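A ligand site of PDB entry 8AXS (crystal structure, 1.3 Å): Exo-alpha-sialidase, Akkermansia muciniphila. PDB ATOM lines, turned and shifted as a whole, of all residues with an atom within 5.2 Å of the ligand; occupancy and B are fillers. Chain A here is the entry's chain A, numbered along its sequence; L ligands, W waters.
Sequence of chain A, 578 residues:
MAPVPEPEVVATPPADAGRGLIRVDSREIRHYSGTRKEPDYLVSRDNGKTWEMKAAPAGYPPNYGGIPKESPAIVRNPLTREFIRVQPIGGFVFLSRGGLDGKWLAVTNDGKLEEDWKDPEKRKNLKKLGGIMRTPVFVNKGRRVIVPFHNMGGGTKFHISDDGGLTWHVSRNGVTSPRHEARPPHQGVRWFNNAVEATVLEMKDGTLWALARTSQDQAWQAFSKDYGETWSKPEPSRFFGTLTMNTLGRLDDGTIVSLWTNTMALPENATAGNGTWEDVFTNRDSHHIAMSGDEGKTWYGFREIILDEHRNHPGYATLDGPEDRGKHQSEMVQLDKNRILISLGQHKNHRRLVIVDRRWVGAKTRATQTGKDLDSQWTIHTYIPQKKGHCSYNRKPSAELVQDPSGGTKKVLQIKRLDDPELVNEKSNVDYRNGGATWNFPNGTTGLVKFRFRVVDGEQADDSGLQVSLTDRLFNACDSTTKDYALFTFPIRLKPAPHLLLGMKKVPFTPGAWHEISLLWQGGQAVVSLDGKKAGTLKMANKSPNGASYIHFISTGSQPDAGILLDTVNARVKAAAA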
ATOM      1  N   ILE A  67      21.235   5.272  23.002  1.00  0.00           N
ATOM      2  CA  ILE A  67      21.721   4.986  21.650  1.00  0.00           C
ATOM      3  C   ILE A  67      22.605   6.125  21.184  1.00  0.00           C
ATOM      4  O   ILE A  67      22.474   7.277  21.641  1.00  0.00           O
ATOM      5  CB  ILE A  67      20.565   4.761  20.653  1.00  0.00           C
ATOM      6  CG1 ILE A  67      19.676   5.986  20.524  1.00  0.00           C
ATOM      7  CG2 ILE A  67      19.740   3.537  21.023  1.00  0.00           C
ATOM      8  CD1 ILE A  67      18.553   5.831  19.476  1.00  0.00           C
ATOM      9  N   LYS A  69      22.844   8.252  18.808  1.00  0.00           N
ATOM     10  CA  LYS A  69      22.382   9.505  18.225  1.00  0.00           C
ATOM     11  C   LYS A  69      21.461  10.320  19.126  1.00  0.00           C
ATOM     12  O   LYS A  69      20.984  11.381  18.718  1.00  0.00           O
ATOM     13  CB  LYS A  69      21.657   9.269  16.879  1.00  0.00           C
ATOM     14  CG  LYS A  69      20.305   8.607  16.985  1.00  0.00           C
ATOM     15  CD  LYS A  69      19.770   8.074  15.647  1.00  0.00           C
ATOM     16  CE  LYS A  69      18.381   7.648  15.749  1.00  0.00           C
ATOM     17  NZ  LYS A  69      17.843   7.478  14.351  1.00  0.00           N
ATOM     18  N   GLU A  70      21.166   9.839  20.320  1.00  0.00           N
ATOM     19  CA  GLU A  70      20.262  10.526  21.244  1.00  0.00           C
ATOM     20  C   GLU A  70      20.911  10.672  22.597  1.00  0.00           C
ATOM     21  O   GLU A  70      21.427   9.704  23.154  1.00  0.00           O
ATOM     22  CB  GLU A  70      18.945   9.761  21.383  1.00  0.00           C
ATOM     23  CG  GLU A  70      18.124   9.800  20.063  1.00  0.00           C
ATOM     24  CD  GLU A  70      16.850   8.944  20.053  1.00  0.00           C
ATOM     25  OE1 GLU A  70      16.485   8.365  21.106  1.00  0.00           O
ATOM     26  OE2 GLU A  70      16.240   8.879  18.920  1.00  0.00           O
ATOM     27  N   ILE A  89      16.204   4.867  26.063  1.00  0.00           N
ATOM     28  CA  ILE A  89      15.915   3.442  26.192  1.00  0.00           C
ATOM     29  C   ILE A  89      17.062   2.801  26.923  1.00  0.00           C
ATOM     30  O   ILE A  89      18.232   3.139  26.699  1.00  0.00           O
ATOM     31  CB  ILE A  89      15.681   2.785  24.800  1.00  0.00           C
ATOM     32  CG1 ILE A  89      15.333   1.318  24.965  1.00  0.00           C
ATOM     33  CG2 ILE A  89      16.890   2.938  23.837  1.00  0.00           C
ATOM     34  CD1 ILE A  89      14.758   0.683  23.721  1.00  0.00           C
ATOM     35  N   ILE A 132      10.558   2.790  25.704  1.00  0.00           N
ATOM     36  CA  ILE A 132      11.163   3.980  25.118  1.00  0.00           C
ATOM     37  C   ILE A 132      10.637   5.185  25.905  1.00  0.00           C
ATOM     38  O   ILE A 132       9.440   5.422  25.938  1.00  0.00           O
ATOM     39  CB  ILE A 132      10.814   4.072  23.631  1.00  0.00           C
ATOM     40  CG1 ILE A 132      11.461   2.891  22.917  1.00  0.00           C
ATOM     41  CG2 ILE A 132      11.277   5.396  23.087  1.00  0.00           C
ATOM     42  CD1 ILE A 132      10.946   2.706  21.482  1.00  0.00           C
ATOM     43  N   HIS A 150       6.793   4.193  26.170  1.00  0.00           N
ATOM     44  CA  HIS A 150       5.937   3.457  25.273  1.00  0.00           C
ATOM     45  C   HIS A 150       6.580   2.199  24.757  1.00  0.00           C
ATOM     46  O   HIS A 150       7.798   2.017  24.773  1.00  0.00           O
ATOM     47  CB  HIS A 150       5.429   4.299  24.090  1.00  0.00           C
ATOM     48  CG  HIS A 150       6.440   4.527  23.005  1.00  0.00           C
ATOM     49  ND1 HIS A 150       7.245   5.647  22.945  1.00  0.00           N
ATOM     50  CD2 HIS A 150       6.771   3.761  21.936  1.00  0.00           C
ATOM     51  CE1 HIS A 150       7.987   5.585  21.840  1.00  0.00           C
ATOM     52  NE2 HIS A 150       7.730   4.438  21.223  1.00  0.00           N
ATOM     53  N   MET A 152       5.775   0.436  20.875  1.00  0.00           N
ATOM     54  CA  MET A 152       5.358   0.949  19.568  1.00  0.00           C
ATOM     55  C   MET A 152       3.907   0.600  19.272  1.00  0.00           C
ATOM     56  O   MET A 152       3.120   1.488  18.920  1.00  0.00           O
ATOM     57  CB  MET A 152       6.305   0.383  18.509  1.00  0.00           C
ATOM     58  CG  MET A 152       5.813   0.354  17.085  1.00  0.00           C
ATOM     59  SD  MET A 152       7.137   0.408  15.871  1.00  0.00           S
ATOM     60  CE  MET A 152       7.234  -1.361  15.642  1.00  0.00           C
ATOM     61  N   TRP A 191       2.290   3.208   8.881  1.00  0.00           N
ATOM     62  CA  TRP A 191       2.982   2.646  10.034  1.00  0.00           C
ATOM     63  C   TRP A 191       2.176   2.893  11.298  1.00  0.00           C
ATOM     64  O   TRP A 191       1.769   4.042  11.569  1.00  0.00           O
ATOM     65  CB  TRP A 191       4.343   3.367  10.127  1.00  0.00           C
ATOM     66  CG  TRP A 191       5.280   2.908  11.242  1.00  0.00           C
ATOM     67  CD1 TRP A 191       5.310   1.672  11.840  1.00  0.00           C
ATOM     68  CD2 TRP A 191       6.341   3.657  11.820  1.00  0.00           C
ATOM     69  NE1 TRP A 191       6.317   1.625  12.779  1.00  0.00           N
ATOM     70  CE2 TRP A 191       6.951   2.845  12.801  1.00  0.00           C
ATOM     71  CE3 TRP A 191       6.813   4.959  11.633  1.00  0.00           C
ATOM     72  CZ2 TRP A 191       8.039   3.272  13.550  1.00  0.00           C
ATOM     73  CZ3 TRP A 191       7.882   5.377  12.391  1.00  0.00           C
ATOM     74  CH2 TRP A 191       8.455   4.552  13.358  1.00  0.00           C
ATOM     75  N   ASN A 193       1.748   3.454  15.051  1.00  0.00           N
ATOM     76  CA  ASN A 193       2.263   3.830  16.360  1.00  0.00           C
ATOM     77  C   ASN A 193       1.056   4.090  17.259  1.00  0.00           C
ATOM     78  O   ASN A 193       0.160   4.867  16.912  1.00  0.00           O
ATOM     79  CB  ASN A 193       3.120   5.119  16.283  1.00  0.00           C
ATOM     80  CG  ASN A 193       4.527   4.933  15.706  1.00  0.00           C
ATOM     81  OD1 ASN A 193       5.295   5.933  15.691  1.00  0.00           O
ATOM     82  ND2 ASN A 193       4.881   3.765  15.207  1.00  0.00           N
ATOM     83  N   VAL A 196       2.403   7.099  20.927  1.00  0.00           N
ATOM     84  CA  VAL A 196       3.768   6.998  21.440  1.00  0.00           C
ATOM     85  C   VAL A 196       4.339   8.385  21.734  1.00  0.00           C
ATOM     86  O   VAL A 196       3.765   9.424  21.396  1.00  0.00           O
ATOM     87  CB  VAL A 196       4.674   6.241  20.442  1.00  0.00           C
ATOM     88  CG1 VAL A 196       4.067   4.845  20.074  1.00  0.00           C
ATOM     89  CG2 VAL A 196       4.907   7.064  19.192  1.00  0.00           C
ATOM     90  N   GLU A 197       5.496   8.402  22.363  1.00  0.00           N
ATOM     91  CA  GLU A 197       6.274   9.641  22.492  1.00  0.00           C
ATOM     92  C   GLU A 197       5.460  10.780  23.117  1.00  0.00           C
ATOM     93  O   GLU A 197       5.411  11.901  22.606  1.00  0.00           O
ATOM     94  CB  GLU A 197       6.934  10.072  21.175  1.00  0.00           C
ATOM     95  CG  GLU A 197       7.944   9.073  20.715  1.00  0.00           C
ATOM     96  CD  GLU A 197       8.610   9.437  19.394  1.00  0.00           C
ATOM     97  OE1 GLU A 197       8.161  10.374  18.686  1.00  0.00           O
ATOM     98  OE2 GLU A 197       9.624   8.727  19.043  1.00  0.00           O
ATOM     99  N   ARG A 213       2.010  11.062  19.740  1.00  0.00           N
ATOM    100  CA  ARG A 213       2.191  10.807  18.307  1.00  0.00           C
ATOM    101  C   ARG A 213       1.429   9.564  17.857  1.00  0.00           C
ATOM    102  O   ARG A 213       1.438   8.511  18.509  1.00  0.00           O
ATOM    103  CB  ARG A 213       3.677  10.517  18.122  1.00  0.00           C
ATOM    104  CG  ARG A 213       4.095   9.807  16.857  1.00  0.00           C
ATOM    105  CD  ARG A 213       5.608   9.707  16.812  1.00  0.00           C
ATOM    106  NE  ARG A 213       6.108   8.611  15.992  1.00  0.00           N
ATOM    107  CZ  ARG A 213       7.375   8.493  15.635  1.00  0.00           C
ATOM    108  NH1 ARG A 213       8.273   9.404  15.988  1.00  0.00           N
ATOM    109  NH2 ARG A 213       7.760   7.438  14.909  1.00  0.00           N
ATOM    110  N   LEU A 243       3.015  10.587  12.979  1.00  0.00           N
ATOM    111  CA  LEU A 243       4.271   9.839  13.126  1.00  0.00           C
ATOM    112  C   LEU A 243       5.483  10.777  13.293  1.00  0.00           C
ATOM    113  O   LEU A 243       6.579  10.493  12.817  1.00  0.00           O
ATOM    114  CB  LEU A 243       4.451   8.830  11.976  1.00  0.00           C
ATOM    115  CG  LEU A 243       3.356   7.759  11.934  1.00  0.00           C
ATOM    116  CD1 LEU A 243       3.289   7.074  10.556  1.00  0.00           C
ATOM    117  CD2 LEU A 243       3.491   6.747  13.054  1.00  0.00           C
ATOM    118  N   TRP A 277       6.168  -1.505  10.282  1.00  0.00           N
ATOM    119  CA  TRP A 277       7.244  -0.538  10.168  1.00  0.00           C
ATOM    120  C   TRP A 277       6.894   0.426   9.025  1.00  0.00           C
ATOM    121  O   TRP A 277       5.917   0.241   8.290  1.00  0.00           O
ATOM    122  CB  TRP A 277       8.606  -1.216   9.908  1.00  0.00           C
ATOM    123  CG  TRP A 277       9.127  -2.061  11.093  1.00  0.00           C
ATOM    124  CD1 TRP A 277       9.189  -3.419  11.159  1.00  0.00           C
ATOM    125  CD2 TRP A 277       9.621  -1.565  12.348  1.00  0.00           C
ATOM    126  NE1 TRP A 277       9.702  -3.807  12.377  1.00  0.00           N
ATOM    127  CE2 TRP A 277       9.968  -2.692  13.129  1.00  0.00           C
ATOM    128  CE3 TRP A 277       9.792  -0.282  12.883  1.00  0.00           C
ATOM    129  CZ2 TRP A 277      10.496  -2.569  14.419  1.00  0.00           C
ATOM    130  CZ3 TRP A 277      10.320  -0.159  14.173  1.00  0.00           C
ATOM    131  CH2 TRP A 277      10.662  -1.293  14.924  1.00  0.00           C
ATOM    132  N   PHE A 281       9.270   8.155   4.617  1.00  0.00           N
ATOM    133  CA  PHE A 281       8.868   9.380   5.287  1.00  0.00           C
ATOM    134  C   PHE A 281       8.690  10.510   4.264  1.00  0.00           C
ATOM    135  O   PHE A 281       9.630  10.868   3.534  1.00  0.00           O
ATOM    136  CB  PHE A 281       9.920   9.794   6.316  1.00  0.00           C
ATOM    137  CG  PHE A 281      10.033   8.892   7.474  1.00  0.00           C
ATOM    138  CD1 PHE A 281       8.967   8.726   8.335  1.00  0.00           C
ATOM    139  CD2 PHE A 281      11.188   8.182   7.717  1.00  0.00           C
ATOM    140  CE1 PHE A 281       9.060   7.906   9.423  1.00  0.00           C
ATOM    141  CE2 PHE A 281      11.297   7.352   8.828  1.00  0.00           C
ATOM    142  CZ  PHE A 281      10.203   7.198   9.654  1.00  0.00           C
ATOM    143  N   ARG A 284       8.618  15.153   7.096  1.00  0.00           N
ATOM    144  CA  ARG A 284       9.482  15.518   8.217  1.00  0.00           C
ATOM    145  C   ARG A 284      10.403  16.691   7.904  1.00  0.00           C
ATOM    146  O   ARG A 284      11.479  16.770   8.488  1.00  0.00           O
ATOM    147  CB  ARG A 284      10.300  14.328   8.688  1.00  0.00           C
ATOM    148  CG  ARG A 284       9.495  13.192   9.326  1.00  0.00           C
ATOM    149  CD  ARG A 284      10.360  12.056   9.819  1.00  0.00           C
ATOM    150  NE  ARG A 284       9.554  11.187  10.667  1.00  0.00           N
ATOM    151  CZ  ARG A 284      10.079  10.318  11.531  1.00  0.00           C
ATOM    152  NH1 ARG A 284      11.379  10.115  11.558  1.00  0.00           N
ATOM    153  NH2 ARG A 284       9.285   9.648  12.344  1.00  0.00           N
ATOM    154  N   ASP A 324      18.141   8.388   9.927  1.00  0.00           N
ATOM    155  CA  ASP A 324      16.949   9.222   9.791  1.00  0.00           C
ATOM    156  C   ASP A 324      17.301  10.702   9.929  1.00  0.00           C
ATOM    157  O   ASP A 324      18.128  11.106  10.758  1.00  0.00           O
ATOM    158  CB  ASP A 324      15.894   8.805  10.805  1.00  0.00           C
ATOM    159  CG  ASP A 324      15.209   7.464  10.422  1.00  0.00           C
ATOM    160  OD1 ASP A 324      15.132   7.126   9.206  1.00  0.00           O
ATOM    161  OD2 ASP A 324      14.716   6.803  11.354  1.00  0.00           O
ATOM    162  N   HIS A 328      11.920  16.954  12.401  1.00  0.00           N
ATOM    163  CA  HIS A 328      11.066  16.445  13.497  1.00  0.00           C
ATOM    164  C   HIS A 328      11.908  16.185  14.746  1.00  0.00           C
ATOM    165  O   HIS A 328      13.120  15.949  14.664  1.00  0.00           O
ATOM    166  CB  HIS A 328      10.199  15.248  12.989  1.00  0.00           C
ATOM    167  CG  HIS A 328      10.337  13.963  13.767  1.00  0.00           C
ATOM    168  ND1 HIS A 328       9.554  13.663  14.886  1.00  0.00           N
ATOM    169  CD2 HIS A 328      11.134  12.893  13.579  1.00  0.00           C
ATOM    170  CE1 HIS A 328       9.857  12.443  15.305  1.00  0.00           C
ATOM    171  NE2 HIS A 328      10.836  11.979  14.556  1.00  0.00           N
ATOM    172  N   GLN A 329      11.227  16.256  15.909  1.00  0.00           N
ATOM    173  CA  GLN A 329      11.732  16.192  17.281  1.00  0.00           C
ATOM    174  C   GLN A 329      12.212  17.552  17.748  1.00  0.00           C
ATOM    175  O   GLN A 329      12.898  18.260  16.988  1.00  0.00           O
ATOM    176  CB  GLN A 329      12.846  15.162  17.514  1.00  0.00           C
ATOM    177  CG  GLN A 329      12.420  13.767  17.077  1.00  0.00           C
ATOM    178  CD  GLN A 329      13.393  12.653  17.370  1.00  0.00           C
ATOM    179  OE1 GLN A 329      13.023  11.488  17.296  1.00  0.00           O
ATOM    180  NE2 GLN A 329      14.667  12.983  17.685  1.00  0.00           N
ATOM    181  N   GLN A 346      16.884  15.796  13.278  1.00  0.00           N
ATOM    182  CA  GLN A 346      17.659  14.575  13.332  1.00  0.00           C
ATOM    183  C   GLN A 346      18.689  14.563  12.209  1.00  0.00           C
ATOM    184  O   GLN A 346      18.423  15.068  11.114  1.00  0.00           O
ATOM    185  CB  GLN A 346      16.753  13.371  13.083  1.00  0.00           C
ATOM    186  CG  GLN A 346      15.691  13.091  14.175  1.00  0.00           C
ATOM    187  CD  GLN A 346      14.752  12.010  13.710  1.00  0.00           C
ATOM    188  OE1 GLN A 346      14.171  12.085  12.620  1.00  0.00           O
ATOM    189  NE2 GLN A 346      14.606  10.981  14.502  1.00  0.00           N
HETATM  190  C1  LIG L   1      11.626   8.309  14.687  1.00  0.00           C
HETATM  191  C2  LIG L   1      12.057   7.659  15.966  1.00  0.00           C
HETATM  192  C3  LIG L   1      13.546   7.713  16.401  1.00  0.00           C
HETATM  193  C4  LIG L   1      13.855   7.100  17.622  1.00  0.00           C
HETATM  194  C5  LIG L   1      12.988   5.738  17.794  1.00  0.00           C
HETATM  195  C6  LIG L   1      11.651   6.044  17.744  1.00  0.00           C
HETATM  196  C7  LIG L   1      10.699   4.854  17.831  1.00  0.00           C
HETATM  197  C8  LIG L   1       9.258   5.338  17.743  1.00  0.00           C
HETATM  198  C9  LIG L   1       8.283   4.120  17.587  1.00  0.00           C
HETATM  199  C10 LIG L   1      13.699   3.740  19.126  1.00  0.00           C
HETATM  200  C11 LIG L   1      14.313   3.250  20.436  1.00  0.00           C
HETATM  201  N1  LIG L   1      13.479   5.183  19.073  1.00  0.00           N
HETATM  202  O1  LIG L   1      12.327   9.176  14.149  1.00  0.00           O
HETATM  203  O2  LIG L   1      10.544   7.893  14.221  1.00  0.00           O
HETATM  204  O3  LIG L   1      15.268   6.798  17.560  1.00  0.00           O
HETATM  205  O4  LIG L   1      11.316   6.589  16.333  1.00  0.00           O
HETATM  206  O5  LIG L   1      10.959   3.932  16.785  1.00  0.00           O
HETATM  207  O6  LIG L   1       8.869   6.013  18.893  1.00  0.00           O
HETATM  208  O7  LIG L   1       8.400   3.231  18.735  1.00  0.00           O
HETATM  209  O8  LIG L   1      13.400   2.986  18.259  1.00  0.00           O
HETATM  210  O   HOH W   1       9.958   0.912  18.247  1.00  0.00           O
HETATM  211  O   HOH W   2      14.248   6.810  21.152  1.00  0.00           O
HETATM  212  O   HOH W   3      12.636   0.404  18.553  1.00  0.00           O
HETATM  213  O   HOH W   4      10.897  10.015  16.925  1.00  0.00           O
HETATM  214  O   HOH W   5      12.175   6.006  12.312  1.00  0.00           O
HETATM  215  O   HOH W   6      15.357   7.449  13.627  1.00  0.00           O
HETATM  216  O   HOH W   7      12.279   4.206  14.209  1.00  0.00           O
HETATM  217  O   HOH W   8      16.439   4.478  16.802  1.00  0.00           O
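OE2 of Glu 197 sits at hydrogen-bond distance from O6 of the ligand, at 2.8 Å. NH2 of Arg 213 is in salt-bridge range of O2 of the ligand, at 2.9 Å. A ring nitrogen (NE2) of His 328 lies within hydrogen-bond range of an oxygen (O1) of the ligand (3.2 Å). O3 of the ligand lies within hydrogen-bond range of OE2 of Glu 70 (2.7 Å). A ring nitrogen (NE2) of His 150 sits at hydrogen-bond distance from an oxygen (O7) of the ligand (2.8 Å). An oxygen (O1) of the ligand sits at hydrogen-bond distance from the side-chain amide nitrogen of Gln 346 (2.9 Å). The guanidinium group of Arg 284 is in salt-bridge range of an oxygen (O2) of the ligand (2.9 Å).
NE1 of Trp 191 is in hydrogen-bond range of SD of Met 152 (3.4 Å). NE of Arg 213 sits at hydrogen-bond distance from OD1 of Asn 193 (2.8 Å). N of His 150 sits at hydrogen-bond distance from O of Ile 132, 2.9 Å away. The guanidinium group of Arg 284 is in hydrogen-bond range of the backbone carbonyl oxygen of Leu 243 (2.9 Å). The side-chain amide nitrogen (NE2) of Gln 346 is in hydrogen-bond range of the side-chain amide oxygen (OE1) of Gln 329, 3.3 Å away. The backbone NH (N) of Glu 197 lies within hydrogen-bond range of a ring nitrogen (ND1) of His 150 (3.3 Å). The backbone carbonyl oxygen of Val 196 lies within hydrogen-bond range of the backbone NH of Arg 213 (2.9 Å). The side-chain carboxylate (OE1) of Glu 197 is in salt-bridge range of the guanidinium group (NH1) of Arg 213.
Residues that only touch the ligand: Ile 67 (3.9 Å), Lys 69 (3.7 Å), Ile 132 (3.6 Å), Met 152 (3.5 Å), Asn 193 (3.98 Å) and Gln 329 (3.9 Å). 13 residues have an atom within 4 Å of the ligand: Ile 67, Lys 69, Glu 70, Ile 132, His 150, Met 152, Asn 193, Glu 197, Arg 213, Arg 284, His 328, Gln 329 and Gln 346. The nearest printed residue that does not touch the ligand is Trp 191 (4.03 Å).
Water W2 lies within hydrogen-bond range of OE1 of Glu 70 (2.7 Å) and N1 of the ligand (2.7 Å). Water W4 lies within hydrogen-bond range of the side-chain amide oxygen (OE1) of Gln 329, the side-chain carboxylate (OE2) of Glu 197, the guanidinium group (NH1) of Arg 213, a ring nitrogen (NE2) of His 328 and an oxygen (O1) of the ligand. Water W1 lies within hydrogen-bond range of O7 of the ligand (2.8 Å) and SD of Met 152 (3.7 Å). Water W5 lies within hydrogen-bond range of OD2 of Asp 324 (2.8 Å) and O2 of the ligand (3.1 Å). Water W6 bridges OD2 of Asp 324 and NZ of Lys 69.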
